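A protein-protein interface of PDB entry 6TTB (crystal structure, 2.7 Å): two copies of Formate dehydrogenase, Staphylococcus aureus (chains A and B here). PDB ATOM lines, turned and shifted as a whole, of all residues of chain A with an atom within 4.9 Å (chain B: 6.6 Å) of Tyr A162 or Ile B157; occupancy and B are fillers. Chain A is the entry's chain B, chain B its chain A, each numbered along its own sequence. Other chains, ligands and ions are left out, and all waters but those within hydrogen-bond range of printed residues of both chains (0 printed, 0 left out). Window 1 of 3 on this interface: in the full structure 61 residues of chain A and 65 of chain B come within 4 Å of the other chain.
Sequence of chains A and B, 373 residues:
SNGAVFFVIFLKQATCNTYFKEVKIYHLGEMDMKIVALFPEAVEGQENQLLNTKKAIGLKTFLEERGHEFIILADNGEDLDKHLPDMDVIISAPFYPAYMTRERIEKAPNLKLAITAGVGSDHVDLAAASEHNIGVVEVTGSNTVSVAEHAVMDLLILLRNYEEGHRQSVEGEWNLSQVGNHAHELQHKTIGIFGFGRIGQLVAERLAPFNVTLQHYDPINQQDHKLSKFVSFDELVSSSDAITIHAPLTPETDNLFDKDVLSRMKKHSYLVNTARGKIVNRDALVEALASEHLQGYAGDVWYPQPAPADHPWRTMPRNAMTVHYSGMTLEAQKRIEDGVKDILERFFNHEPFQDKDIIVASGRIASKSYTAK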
ATOM      1  N   MET A 153      -6.042   2.550  10.635  1.00  0.00           N
ATOM      2  CA  MET A 153      -5.724   1.295  11.283  1.00  0.00           C
ATOM      3  C   MET A 153      -4.919   0.434  10.313  1.00  0.00           C
ATOM      4  O   MET A 153      -3.875  -0.110  10.676  1.00  0.00           O
ATOM      5  CB  MET A 153      -7.014   0.565  11.684  1.00  0.00           C
ATOM      6  CG  MET A 153      -6.781  -0.794  12.297  1.00  0.00           C
ATOM      7  SD  MET A 153      -8.375  -1.768  12.446  1.00  0.00           S
ATOM      8  CE  MET A 153      -8.788  -2.149  10.742  1.00  0.00           C
ATOM      9  N   ILE A 157      -1.410  -1.218  11.007  1.00  0.00           N
ATOM     10  CA  ILE A 157      -1.193  -2.646  10.922  1.00  0.00           C
ATOM     11  C   ILE A 157      -0.082  -2.947   9.947  1.00  0.00           C
ATOM     12  O   ILE A 157       0.765  -3.794  10.214  1.00  0.00           O
ATOM     13  CB  ILE A 157      -2.450  -3.378  10.477  1.00  0.00           C
ATOM     14  CG1 ILE A 157      -3.572  -3.316  11.521  1.00  0.00           C
ATOM     15  CG2 ILE A 157      -2.111  -4.806  10.083  1.00  0.00           C
ATOM     16  CD1 ILE A 157      -4.854  -3.846  11.030  1.00  0.00           C
ATOM     17  N   ARG A 160       3.955  -0.756  11.278  1.00  0.00           N
ATOM     18  CA  ARG A 160       4.167  -1.669  12.383  1.00  0.00           C
ATOM     19  C   ARG A 160       3.779  -3.013  11.801  1.00  0.00           C
ATOM     20  O   ARG A 160       2.881  -3.059  10.947  1.00  0.00           O
ATOM     21  CB  ARG A 160       3.214  -1.302  13.526  1.00  0.00           C
ATOM     22  CG  ARG A 160       3.127   0.191  13.840  1.00  0.00           C
ATOM     23  CD  ARG A 160       2.646   0.546  15.254  1.00  0.00           C
ATOM     24  NE  ARG A 160       3.522   0.011  16.270  1.00  0.00           N
ATOM     25  CZ  ARG A 160       4.613   0.684  16.700  1.00  0.00           C
ATOM     26  NH1 ARG A 160       4.857   1.898  16.230  1.00  0.00           N
ATOM     27  NH2 ARG A 160       5.395   0.199  17.671  1.00  0.00           N
ATOM     28  N   ASN A 161       4.486  -4.072  12.159  1.00  0.00           N
ATOM     29  CA  ASN A 161       4.347  -5.249  11.325  1.00  0.00           C
ATOM     30  C   ASN A 161       3.321  -6.191  12.000  1.00  0.00           C
ATOM     31  O   ASN A 161       3.613  -7.360  12.308  1.00  0.00           O
ATOM     32  CB  ASN A 161       5.735  -5.613  10.857  1.00  0.00           C
ATOM     33  CG  ASN A 161       5.953  -6.986  10.315  1.00  0.00           C
ATOM     34  OD1 ASN A 161       5.216  -7.429   9.462  1.00  0.00           O
ATOM     35  ND2 ASN A 161       7.113  -7.543  10.596  1.00  0.00           N
ATOM     36  N   TYR A 162       2.127  -5.629  12.327  1.00  0.00           N
ATOM     37  CA  TYR A 162       1.200  -6.286  13.249  1.00  0.00           C
ATOM     38  C   TYR A 162       0.862  -7.695  12.790  1.00  0.00           C
ATOM     39  O   TYR A 162       0.602  -8.563  13.592  1.00  0.00           O
ATOM     40  CB  TYR A 162      -0.106  -5.534  13.406  1.00  0.00           C
ATOM     41  CG  TYR A 162      -1.161  -6.324  14.153  1.00  0.00           C
ATOM     42  CD1 TYR A 162      -1.191  -6.369  15.555  1.00  0.00           C
ATOM     43  CD2 TYR A 162      -2.157  -7.014  13.468  1.00  0.00           C
ATOM     44  CE1 TYR A 162      -2.159  -7.099  16.230  1.00  0.00           C
ATOM     45  CE2 TYR A 162      -3.097  -7.795  14.120  1.00  0.00           C
ATOM     46  CZ  TYR A 162      -3.098  -7.841  15.504  1.00  0.00           C
ATOM     47  OH  TYR A 162      -4.057  -8.564  16.144  1.00  0.00           O
ATOM     48  N   GLU A 163       0.767  -7.914  11.518  1.00  0.00           N
ATOM     49  CA  GLU A 163       0.296  -9.222  11.073  1.00  0.00           C
ATOM     50  C   GLU A 163       1.285 -10.324  11.519  1.00  0.00           C
ATOM     51  O   GLU A 163       0.904 -11.371  12.033  1.00  0.00           O
ATOM     52  CB  GLU A 163       0.073  -9.189   9.564  1.00  0.00           C
ATOM     53  CG  GLU A 163      -1.317  -8.771   9.215  1.00  0.00           C
ATOM     54  CD  GLU A 163      -2.339  -9.830   9.547  1.00  0.00           C
ATOM     55  OE1 GLU A 163      -2.123 -11.052   9.131  1.00  0.00           O
ATOM     56  OE2 GLU A 163      -3.331  -9.490  10.254  1.00  0.00           O
ATOM     57  N   GLU A 164       2.563 -10.058  11.308  1.00  0.00           N
ATOM     58  CA  GLU A 164       3.603 -11.004  11.658  1.00  0.00           C
ATOM     59  C   GLU A 164       3.677 -11.044  13.180  1.00  0.00           C
ATOM     60  O   GLU A 164       3.834 -12.115  13.788  1.00  0.00           O
ATOM     61  CB  GLU A 164       4.956 -10.567  11.079  1.00  0.00           C
ATOM     62  CG  GLU A 164       6.061 -11.440  11.505  1.00  0.00           C
ATOM     63  CD  GLU A 164       5.878 -12.878  11.101  1.00  0.00           C
ATOM     64  OE1 GLU A 164       4.863 -13.158  10.384  1.00  0.00           O
ATOM     65  OE2 GLU A 164       6.702 -13.724  11.518  1.00  0.00           O
ATOM     66  N   GLY A 165       3.558  -9.858  13.781  1.00  0.00           N
ATOM     67  CA  GLY A 165       3.605  -9.741  15.228  1.00  0.00           C
ATOM     68  C   GLY A 165       2.573 -10.631  15.880  1.00  0.00           C
ATOM     69  O   GLY A 165       2.843 -11.205  16.944  1.00  0.00           O
ATOM     70  N   HIS A 166       1.407 -10.762  15.225  1.00  0.00           N
ATOM     71  CA  HIS A 166       0.302 -11.516  15.802  1.00  0.00           C
ATOM     72  C   HIS A 166       0.417 -12.997  15.462  1.00  0.00           C
ATOM     73  O   HIS A 166       0.071 -13.842  16.271  1.00  0.00           O
ATOM     74  CB  HIS A 166      -1.051 -10.891  15.426  1.00  0.00           C
ATOM     75  CG  HIS A 166      -2.232 -11.627  15.945  1.00  0.00           C
ATOM     76  ND1 HIS A 166      -2.483 -11.753  17.280  1.00  0.00           N
ATOM     77  CD2 HIS A 166      -3.218 -12.285  15.315  1.00  0.00           C
ATOM     78  CE1 HIS A 166      -3.608 -12.451  17.464  1.00  0.00           C
ATOM     79  NE2 HIS A 166      -4.089 -12.762  16.265  1.00  0.00           N
ATOM     80  N   ARG A 167       0.860 -13.304  14.239  1.00  0.00           N
ATOM     81  CA  ARG A 167       1.057 -14.683  13.837  1.00  0.00           C
ATOM     82  C   ARG A 167       2.018 -15.360  14.817  1.00  0.00           C
ATOM     83  O   ARG A 167       1.658 -16.351  15.453  1.00  0.00           O
ATOM     84  CB  ARG A 167       1.542 -14.757  12.391  1.00  0.00           C
ATOM     85  CG  ARG A 167       1.551 -16.184  11.836  1.00  0.00           C
ATOM     86  CD  ARG A 167       2.580 -16.367  10.721  1.00  0.00           C
ATOM     87  NE  ARG A 167       3.959 -16.016  11.071  1.00  0.00           N
ATOM     88  CZ  ARG A 167       4.745 -16.793  11.813  1.00  0.00           C
ATOM     89  NH1 ARG A 167       4.289 -17.964  12.232  1.00  0.00           N
ATOM     90  NH2 ARG A 167       5.964 -16.383  12.185  1.00  0.00           N
ATOM     91  N   HIS B 150       1.544   1.791  18.846  1.00  0.00           N
ATOM     92  CA  HIS B 150       1.075   0.423  18.977  1.00  0.00           C
ATOM     93  C   HIS B 150      -0.224   0.401  19.779  1.00  0.00           C
ATOM     94  O   HIS B 150      -1.098  -0.419  19.538  1.00  0.00           O
ATOM     95  CB  HIS B 150       2.099  -0.385  19.685  1.00  0.00           C
ATOM     96  CG  HIS B 150       2.061  -1.792  19.279  1.00  0.00           C
ATOM     97  ND1 HIS B 150       2.796  -2.270  18.184  1.00  0.00           N
ATOM     98  CD2 HIS B 150       1.411  -2.852  19.812  1.00  0.00           C
ATOM     99  CE1 HIS B 150       2.613  -3.578  18.092  1.00  0.00           C
ATOM    100  NE2 HIS B 150       1.772  -3.956  19.090  1.00  0.00           N
ATOM    101  N   VAL B 152      -2.682   2.753  20.114  1.00  0.00           N
ATOM    102  CA  VAL B 152      -3.882   3.263  19.468  1.00  0.00           C
ATOM    103  C   VAL B 152      -4.277   2.276  18.394  1.00  0.00           C
ATOM    104  O   VAL B 152      -5.469   1.970  18.241  1.00  0.00           O
ATOM    105  CB  VAL B 152      -3.781   4.735  18.993  1.00  0.00           C
ATOM    106  CG1 VAL B 152      -3.373   5.655  20.124  1.00  0.00           C
ATOM    107  CG2 VAL B 152      -2.801   4.878  17.951  1.00  0.00           C
ATOM    108  N   MET B 153      -3.271   1.606  17.822  1.00  0.00           N
ATOM    109  CA  MET B 153      -3.552   0.568  16.827  1.00  0.00           C
ATOM    110  C   MET B 153      -4.369  -0.542  17.478  1.00  0.00           C
ATOM    111  O   MET B 153      -5.441  -0.942  16.967  1.00  0.00           O
ATOM    112  CB  MET B 153      -2.268  -0.018  16.300  1.00  0.00           C
ATOM    113  CG  MET B 153      -2.438  -1.162  15.395  1.00  0.00           C
ATOM    114  SD  MET B 153      -0.797  -1.818  14.954  1.00  0.00           S
ATOM    115  CE  MET B 153      -0.415  -2.810  16.411  1.00  0.00           C
ATOM    116  N   ASP B 154      -3.907  -0.960  18.654  1.00  0.00           N
ATOM    117  CA  ASP B 154      -4.630  -1.930  19.455  1.00  0.00           C
ATOM    118  C   ASP B 154      -6.055  -1.470  19.735  1.00  0.00           C
ATOM    119  O   ASP B 154      -6.972  -2.302  19.624  1.00  0.00           O
ATOM    120  CB  ASP B 154      -3.887  -2.277  20.742  1.00  0.00           C
ATOM    121  CG  ASP B 154      -2.571  -3.041  20.577  1.00  0.00           C
ATOM    122  OD1 ASP B 154      -2.318  -3.560  19.551  1.00  0.00           O
ATOM    123  OD2 ASP B 154      -1.885  -3.162  21.537  1.00  0.00           O
ATOM    124  N   LEU B 155      -6.262  -0.192  20.168  1.00  0.00           N
ATOM    125  CA  LEU B 155      -7.650   0.282  20.352  1.00  0.00           C
ATOM    126  C   LEU B 155      -8.428  -0.016  19.092  1.00  0.00           C
ATOM    127  O   LEU B 155      -9.390  -0.727  19.132  1.00  0.00           O
ATOM    128  CB  LEU B 155      -7.744   1.787  20.624  1.00  0.00           C
ATOM    129  CG  LEU B 155      -7.720   2.266  22.092  1.00  0.00           C
ATOM    130  CD1 LEU B 155      -8.092   1.141  23.095  1.00  0.00           C
ATOM    131  CD2 LEU B 155      -6.370   2.799  22.398  1.00  0.00           C
ATOM    132  N   LEU B 156      -7.919   0.459  17.956  1.00  0.00           N
ATOM    133  CA  LEU B 156      -8.609   0.335  16.705  1.00  0.00           C
ATOM    134  C   LEU B 156      -8.879  -1.131  16.394  1.00  0.00           C
ATOM    135  O   LEU B 156     -10.000  -1.488  16.161  1.00  0.00           O
ATOM    136  CB  LEU B 156      -7.766   1.024  15.628  1.00  0.00           C
ATOM    137  CG  LEU B 156      -7.755   2.560  15.699  1.00  0.00           C
ATOM    138  CD1 LEU B 156      -6.599   3.142  14.924  1.00  0.00           C
ATOM    139  CD2 LEU B 156      -9.053   3.152  15.184  1.00  0.00           C
ATOM    140  N   ILE B 157      -7.855  -1.989  16.419  1.00  0.00           N
ATOM    141  CA  ILE B 157      -8.034  -3.406  16.064  1.00  0.00           C
ATOM    142  C   ILE B 157      -9.107  -4.006  16.958  1.00  0.00           C
ATOM    143  O   ILE B 157      -9.909  -4.791  16.534  1.00  0.00           O
ATOM    144  CB  ILE B 157      -6.703  -4.183  16.213  1.00  0.00           C
ATOM    145  CG1 ILE B 157      -5.670  -3.760  15.177  1.00  0.00           C
ATOM    146  CG2 ILE B 157      -6.932  -5.698  16.205  1.00  0.00           C
ATOM    147  CD1 ILE B 157      -4.341  -4.434  15.342  1.00  0.00           C
ATOM    148  N   LEU B 158      -9.055  -3.680  18.221  1.00  0.00           N
ATOM    149  CA  LEU B 158     -10.016  -4.183  19.173  1.00  0.00           C
ATOM    150  C   LEU B 158     -11.455  -3.699  18.860  1.00  0.00           C
ATOM    151  O   LEU B 158     -12.374  -4.508  18.719  1.00  0.00           O
ATOM    152  CB  LEU B 158      -9.499  -3.779  20.556  1.00  0.00           C
ATOM    153  CG  LEU B 158      -8.816  -4.923  21.366  1.00  0.00           C
ATOM    154  CD1 LEU B 158      -8.389  -6.106  20.496  1.00  0.00           C
ATOM    155  CD2 LEU B 158      -7.637  -4.448  22.154  1.00  0.00           C
ATOM    156  N   LEU B 159     -11.687  -2.381  18.783  1.00  0.00           N
ATOM    157  CA  LEU B 159     -13.059  -1.889  18.623  1.00  0.00           C
ATOM    158  C   LEU B 159     -13.582  -2.254  17.240  1.00  0.00           C
ATOM    159  O   LEU B 159     -14.731  -2.585  17.065  1.00  0.00           O
ATOM    160  CB  LEU B 159     -13.134  -0.371  18.850  1.00  0.00           C
ATOM    161  CG  LEU B 159     -13.158   0.039  20.326  1.00  0.00           C
ATOM    162  CD1 LEU B 159     -12.267   1.240  20.525  1.00  0.00           C
ATOM    163  CD2 LEU B 159     -14.570   0.311  20.839  1.00  0.00           C
ATOM    164  N   ARG B 160     -12.714  -2.232  16.259  1.00  0.00           N
ATOM    165  CA  ARG B 160     -13.202  -2.397  14.911  1.00  0.00           C
ATOM    166  C   ARG B 160     -13.323  -3.877  14.615  1.00  0.00           C
ATOM    167  O   ARG B 160     -13.892  -4.259  13.588  1.00  0.00           O
ATOM    168  CB  ARG B 160     -12.347  -1.605  13.913  1.00  0.00           C
ATOM    169  CG  ARG B 160     -12.536  -0.111  14.056  1.00  0.00           C
ATOM    170  CD  ARG B 160     -12.145   0.663  12.833  1.00  0.00           C
ATOM    171  NE  ARG B 160     -12.946   0.372  11.663  1.00  0.00           N
ATOM    172  CZ  ARG B 160     -14.034   1.043  11.355  1.00  0.00           C
ATOM    173  NH1 ARG B 160     -14.486   1.986  12.186  1.00  0.00           N
ATOM    174  NH2 ARG B 160     -14.666   0.774  10.218  1.00  0.00           N
ATOM    175  N   ASN B 161     -12.850  -4.715  15.553  1.00  0.00           N
ATOM    176  CA  ASN B 161     -13.020  -6.135  15.361  1.00  0.00           C
ATOM    177  C   ASN B 161     -12.297  -6.532  14.056  1.00  0.00           C
ATOM    178  O   ASN B 161     -12.750  -7.380  13.276  1.00  0.00           O
ATOM    179  CB  ASN B 161     -14.529  -6.462  15.411  1.00  0.00           C
ATOM    180  CG  ASN B 161     -14.857  -7.941  15.376  1.00  0.00           C
ATOM    181  OD1 ASN B 161     -14.131  -8.794  15.910  1.00  0.00           O
ATOM    182  ND2 ASN B 161     -15.947  -8.259  14.715  1.00  0.00           N
ATOM    183  N   TYR B 162     -11.165  -5.876  13.806  1.00  0.00           N
ATOM    184  CA  TYR B 162     -10.273  -6.230  12.722  1.00  0.00           C
ATOM    185  C   TYR B 162     -10.015  -7.730  12.672  1.00  0.00           C
ATOM    186  O   TYR B 162      -9.805  -8.285  11.615  1.00  0.00           O
ATOM    187  CB  TYR B 162      -8.942  -5.537  12.904  1.00  0.00           C
ATOM    188  CG  TYR B 162      -7.891  -6.006  11.939  1.00  0.00           C
ATOM    189  CD1 TYR B 162      -7.883  -5.578  10.615  1.00  0.00           C
ATOM    190  CD2 TYR B 162      -6.966  -6.960  12.329  1.00  0.00           C
ATOM    191  CE1 TYR B 162      -6.978  -6.101   9.690  1.00  0.00           C
ATOM    192  CE2 TYR B 162      -6.068  -7.517  11.432  1.00  0.00           C
ATOM    193  CZ  TYR B 162      -6.055  -7.057  10.115  1.00  0.00           C
ATOM    194  OH  TYR B 162      -5.089  -7.504   9.291  1.00  0.00           O
ATOM    195  N   GLU B 163      -9.951  -8.378  13.827  1.00  0.00           N
ATOM    196  CA  GLU B 163      -9.488  -9.756  13.811  1.00  0.00           C
ATOM    197  C   GLU B 163     -10.463 -10.613  13.053  1.00  0.00           C
ATOM    198  O   GLU B 163     -10.071 -11.443  12.268  1.00  0.00           O
ATOM    199  CB  GLU B 163      -9.293 -10.307  15.208  1.00  0.00           C
ATOM    200  CG  GLU B 163      -7.929 -10.007  15.743  1.00  0.00           C
ATOM    201  CD  GLU B 163      -6.782 -10.588  14.951  1.00  0.00           C
ATOM    202  OE1 GLU B 163      -6.848 -11.805  14.590  1.00  0.00           O
ATOM    203  OE2 GLU B 163      -5.831  -9.834  14.694  1.00  0.00           O
ATOM    204  N   TYR B 270     -12.885  -2.959  26.694  1.00  0.00           N
ATOM    205  CA  TYR B 270     -11.649  -3.495  26.122  1.00  0.00           C
ATOM    206  C   TYR B 270     -10.461  -2.994  26.940  1.00  0.00           C
ATOM    207  O   TYR B 270     -10.507  -1.903  27.492  1.00  0.00           O
ATOM    208  CB  TYR B 270     -11.444  -3.016  24.672  1.00  0.00           C
ATOM    209  CG  TYR B 270     -12.562  -3.314  23.728  1.00  0.00           C
ATOM    210  CD1 TYR B 270     -13.754  -2.574  23.732  1.00  0.00           C
ATOM    211  CD2 TYR B 270     -12.420  -4.314  22.783  1.00  0.00           C
ATOM    212  CE1 TYR B 270     -14.775  -2.837  22.831  1.00  0.00           C
ATOM    213  CE2 TYR B 270     -13.430  -4.579  21.868  1.00  0.00           C
ATOM    214  CZ  TYR B 270     -14.617  -3.850  21.901  1.00  0.00           C
ATOM    215  OH  TYR B 270     -15.592  -4.176  20.991  1.00  0.00           O
ATOM    216  N   ALA B 298      -5.732  -6.418  23.956  1.00  0.00           N
ATOM    217  CA  ALA B 298      -4.500  -6.377  23.181  1.00  0.00           C
ATOM    218  C   ALA B 298      -3.382  -5.765  23.993  1.00  0.00           C
ATOM    219  O   ALA B 298      -3.598  -5.313  25.134  1.00  0.00           O
ATOM    220  CB  ALA B 298      -4.660  -5.650  21.876  1.00  0.00           C
ATOM    221  N   ASN B 319      -8.197 -12.007  21.419  1.00  0.00           N
ATOM    222  CA  ASN B 319      -6.949 -11.318  21.750  1.00  0.00           C
ATOM    223  C   ASN B 319      -6.359 -10.677  20.507  1.00  0.00           C
ATOM    224  O   ASN B 319      -6.592 -11.184  19.398  1.00  0.00           O
ATOM    225  CB  ASN B 319      -5.925 -12.232  22.468  1.00  0.00           C
ATOM    226  CG  ASN B 319      -5.045 -13.010  21.535  1.00  0.00           C
ATOM    227  OD1 ASN B 319      -4.084 -12.475  21.032  1.00  0.00           O
ATOM    228  ND2 ASN B 319      -5.341 -14.282  21.332  1.00  0.00           N
ATOM    229  N   ALA B 320      -5.639  -9.526  20.693  1.00  0.00           N
ATOM    230  CA  ALA B 320      -4.747  -8.990  19.665  1.00  0.00           C
ATOM    231  C   ALA B 320      -3.345  -8.768  20.226  1.00  0.00           C
ATOM    232  O   ALA B 320      -2.720  -7.662  20.148  1.00  0.00           O
ATOM    233  CB  ALA B 320      -5.315  -7.794  19.001  1.00  0.00           C
ATOM    234  N   MET B 321      -2.832  -9.854  20.793  1.00  0.00           N
ATOM    235  CA  MET B 321      -1.486  -9.844  21.275  1.00  0.00           C
ATOM    236  C   MET B 321      -0.593  -9.797  20.050  1.00  0.00           C
ATOM    237  O   MET B 321      -1.024 -10.075  18.936  1.00  0.00           O
ATOM    238  CB  MET B 321      -1.194 -11.130  22.062  1.00  0.00           C
ATOM    239  CG  MET B 321      -1.996 -11.280  23.391  1.00  0.00           C
ATOM    240  SD  MET B 321      -1.769  -9.874  24.448  1.00  0.00           S
ATOM    241  CE  MET B 321       0.022  -9.718  24.490  1.00  0.00           C
ATOM    242  N   THR B 322       0.570  -9.257  20.240  1.00  0.00           N
ATOM    243  CA  THR B 322       1.699  -9.574  19.443  1.00  0.00           C
ATOM    244  C   THR B 322       2.826  -9.954  20.419  1.00  0.00           C
ATOM    245  O   THR B 322       2.753  -9.723  21.628  1.00  0.00           O
ATOM    246  CB  THR B 322       2.055  -8.347  18.609  1.00  0.00           C
ATOM    247  OG1 THR B 322       2.615  -7.300  19.416  1.00  0.00           O
ATOM    248  CG2 THR B 322       0.881  -7.811  17.810  1.00  0.00           C
ATOM    249  N   TYR B 325       7.585  -6.388  20.499  1.00  0.00           N
ATOM    250  CA  TYR B 325       8.510  -5.604  19.699  1.00  0.00           C
ATOM    251  C   TYR B 325       8.097  -4.130  19.530  1.00  0.00           C
ATOM    252  O   TYR B 325       8.763  -3.397  18.811  1.00  0.00           O
ATOM    253  CB  TYR B 325       8.562  -6.222  18.316  1.00  0.00           C
ATOM    254  CG  TYR B 325       7.300  -6.007  17.542  1.00  0.00           C
ATOM    255  CD1 TYR B 325       6.155  -6.741  17.801  1.00  0.00           C
ATOM    256  CD2 TYR B 325       7.239  -5.021  16.558  1.00  0.00           C
ATOM    257  CE1 TYR B 325       5.015  -6.551  17.029  1.00  0.00           C
ATOM    258  CE2 TYR B 325       6.104  -4.812  15.809  1.00  0.00           C
ATOM    259  CZ  TYR B 325       5.014  -5.607  16.020  1.00  0.00           C
ATOM    260  OH  TYR B 325       3.932  -5.342  15.277  1.00  0.00           O
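Met A153 touches Ile B157, but with the chains exchanged Ile A157 does not touch Met B153 (4.04 Å).
Met A153 touches Tyr B162, and with the chains exchanged Tyr A162 touches Met B153.
Ile A157 touches Tyr B162, and with the chains exchanged Tyr A162 touches Ile B157.
Tyr A162 touches Glu B163, and with the chains exchanged Glu A163 touches Tyr B162.
Positions printed for both chains: 153, 157, 160, 161, 162 and 163.
ND1 of His B150 is in hydrogen-bond range of NE of Arg A160 (3.1 Å).
The side-chain hydroxyl (OH) of Tyr B162 is in hydrogen-bond range of the side-chain carboxylate (OE2) of Glu A163 (2.8 Å).
The side-chain carboxylate (OE2) of Glu B163 is in hydrogen-bond range of the side-chain hydroxyl (OH) of Tyr A162 (2.6 Å).
OE1 of Glu B163 sits at hydrogen-bond distance from NE2 of His A166, 3.4 Å away.
The backbone carbonyl oxygen (O) of Met B321 lies within hydrogen-bond range of a ring nitrogen (ND1) of His A166, 2.8 Å away.
The backbone NH (N) of Asn A161 lies within hydrogen-bond range of the side-chain hydroxyl (OH) of Tyr B325 (3.4 Å).
OH of Tyr B325 lies within hydrogen-bond range of N of Tyr A162, at 3.5 Å.
Of the 10 printed residues of chain A, 8 touch a printed residue of chain B.
Hydrophobic or aromatic side chains of chain A within 4 Å of the printed part of chain B: Met A153, Ile A157, Tyr A162 and His A166.
Along chain A the printed residues that touch a printed residue of chain B span positions 153 to 166.
Among the printed residues, 19 pairs touch across the chains.
Of the printed residues of chain B, Tyr A162 touches Met B153, Ile B157, Glu B163, Ala B320, Thr B322 and Tyr B325.
Of the printed residues of chain A, Ile B157 touches Met A153 and Tyr A162.
Printed residues of chain A within 4 Å of Met B321: His A166 (2.8 Å).
Of the printed residues of chain B, Met A153 touches Leu B156 (3.9 Å), Ile B157 (3.99 Å) and Tyr B162 (3.5 Å).
Of the printed residues of chain B, Arg A160 touches His B150.
Printed residues of chain B within 4 Å of Glu A163: Tyr B162.
Leu B158 touches none of the printed residues of chain A.
Ala B298 touches none of the printed residues of chain A.
The nearest printed residue of chain A that does not touch Ile B157 is Ile A157 (4.1 Å).
The nearest printed residue of chain A that does not touch His B150 is Tyr A162 (5.2 Å).
OG1 of Thr B322 sits at hydrogen-bond distance from NE2 of His B150, 3.5 Å away.
N of Tyr B162 lies within hydrogen-bond range of O of Ile B157, 3.2 Å away.
OD1 of Asn B319 sits at hydrogen-bond distance from N of Met B321 (2.9 Å).
The backbone carbonyl oxygen (O) of Ile A157 is in hydrogen-bond range of the backbone NH (N) of Tyr A162.
Among the printed residues, pairs that only touch across the chains: Gly A165 with Thr B322 (3.2 Å), Tyr A162 with Ala B320 (3.2 Å), Ile A157 with Tyr B162 (3.4 Å), Tyr A162 with Thr B322 (3.4 Å), Met A153 with Tyr B162 (3.5 Å), Tyr A162 with Ile B157 (3.6 Å), His A166 with Asn B319 (3.6 Å), Tyr A162 with Met B153 (3.7 Å), Met A153 with Leu B156 (3.9 Å), Gly A165 with Tyr B325 (3.9 Å), His A166 with Thr B322 (3.96 Å) and Met A153 with Ile B157 (3.99 Å).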
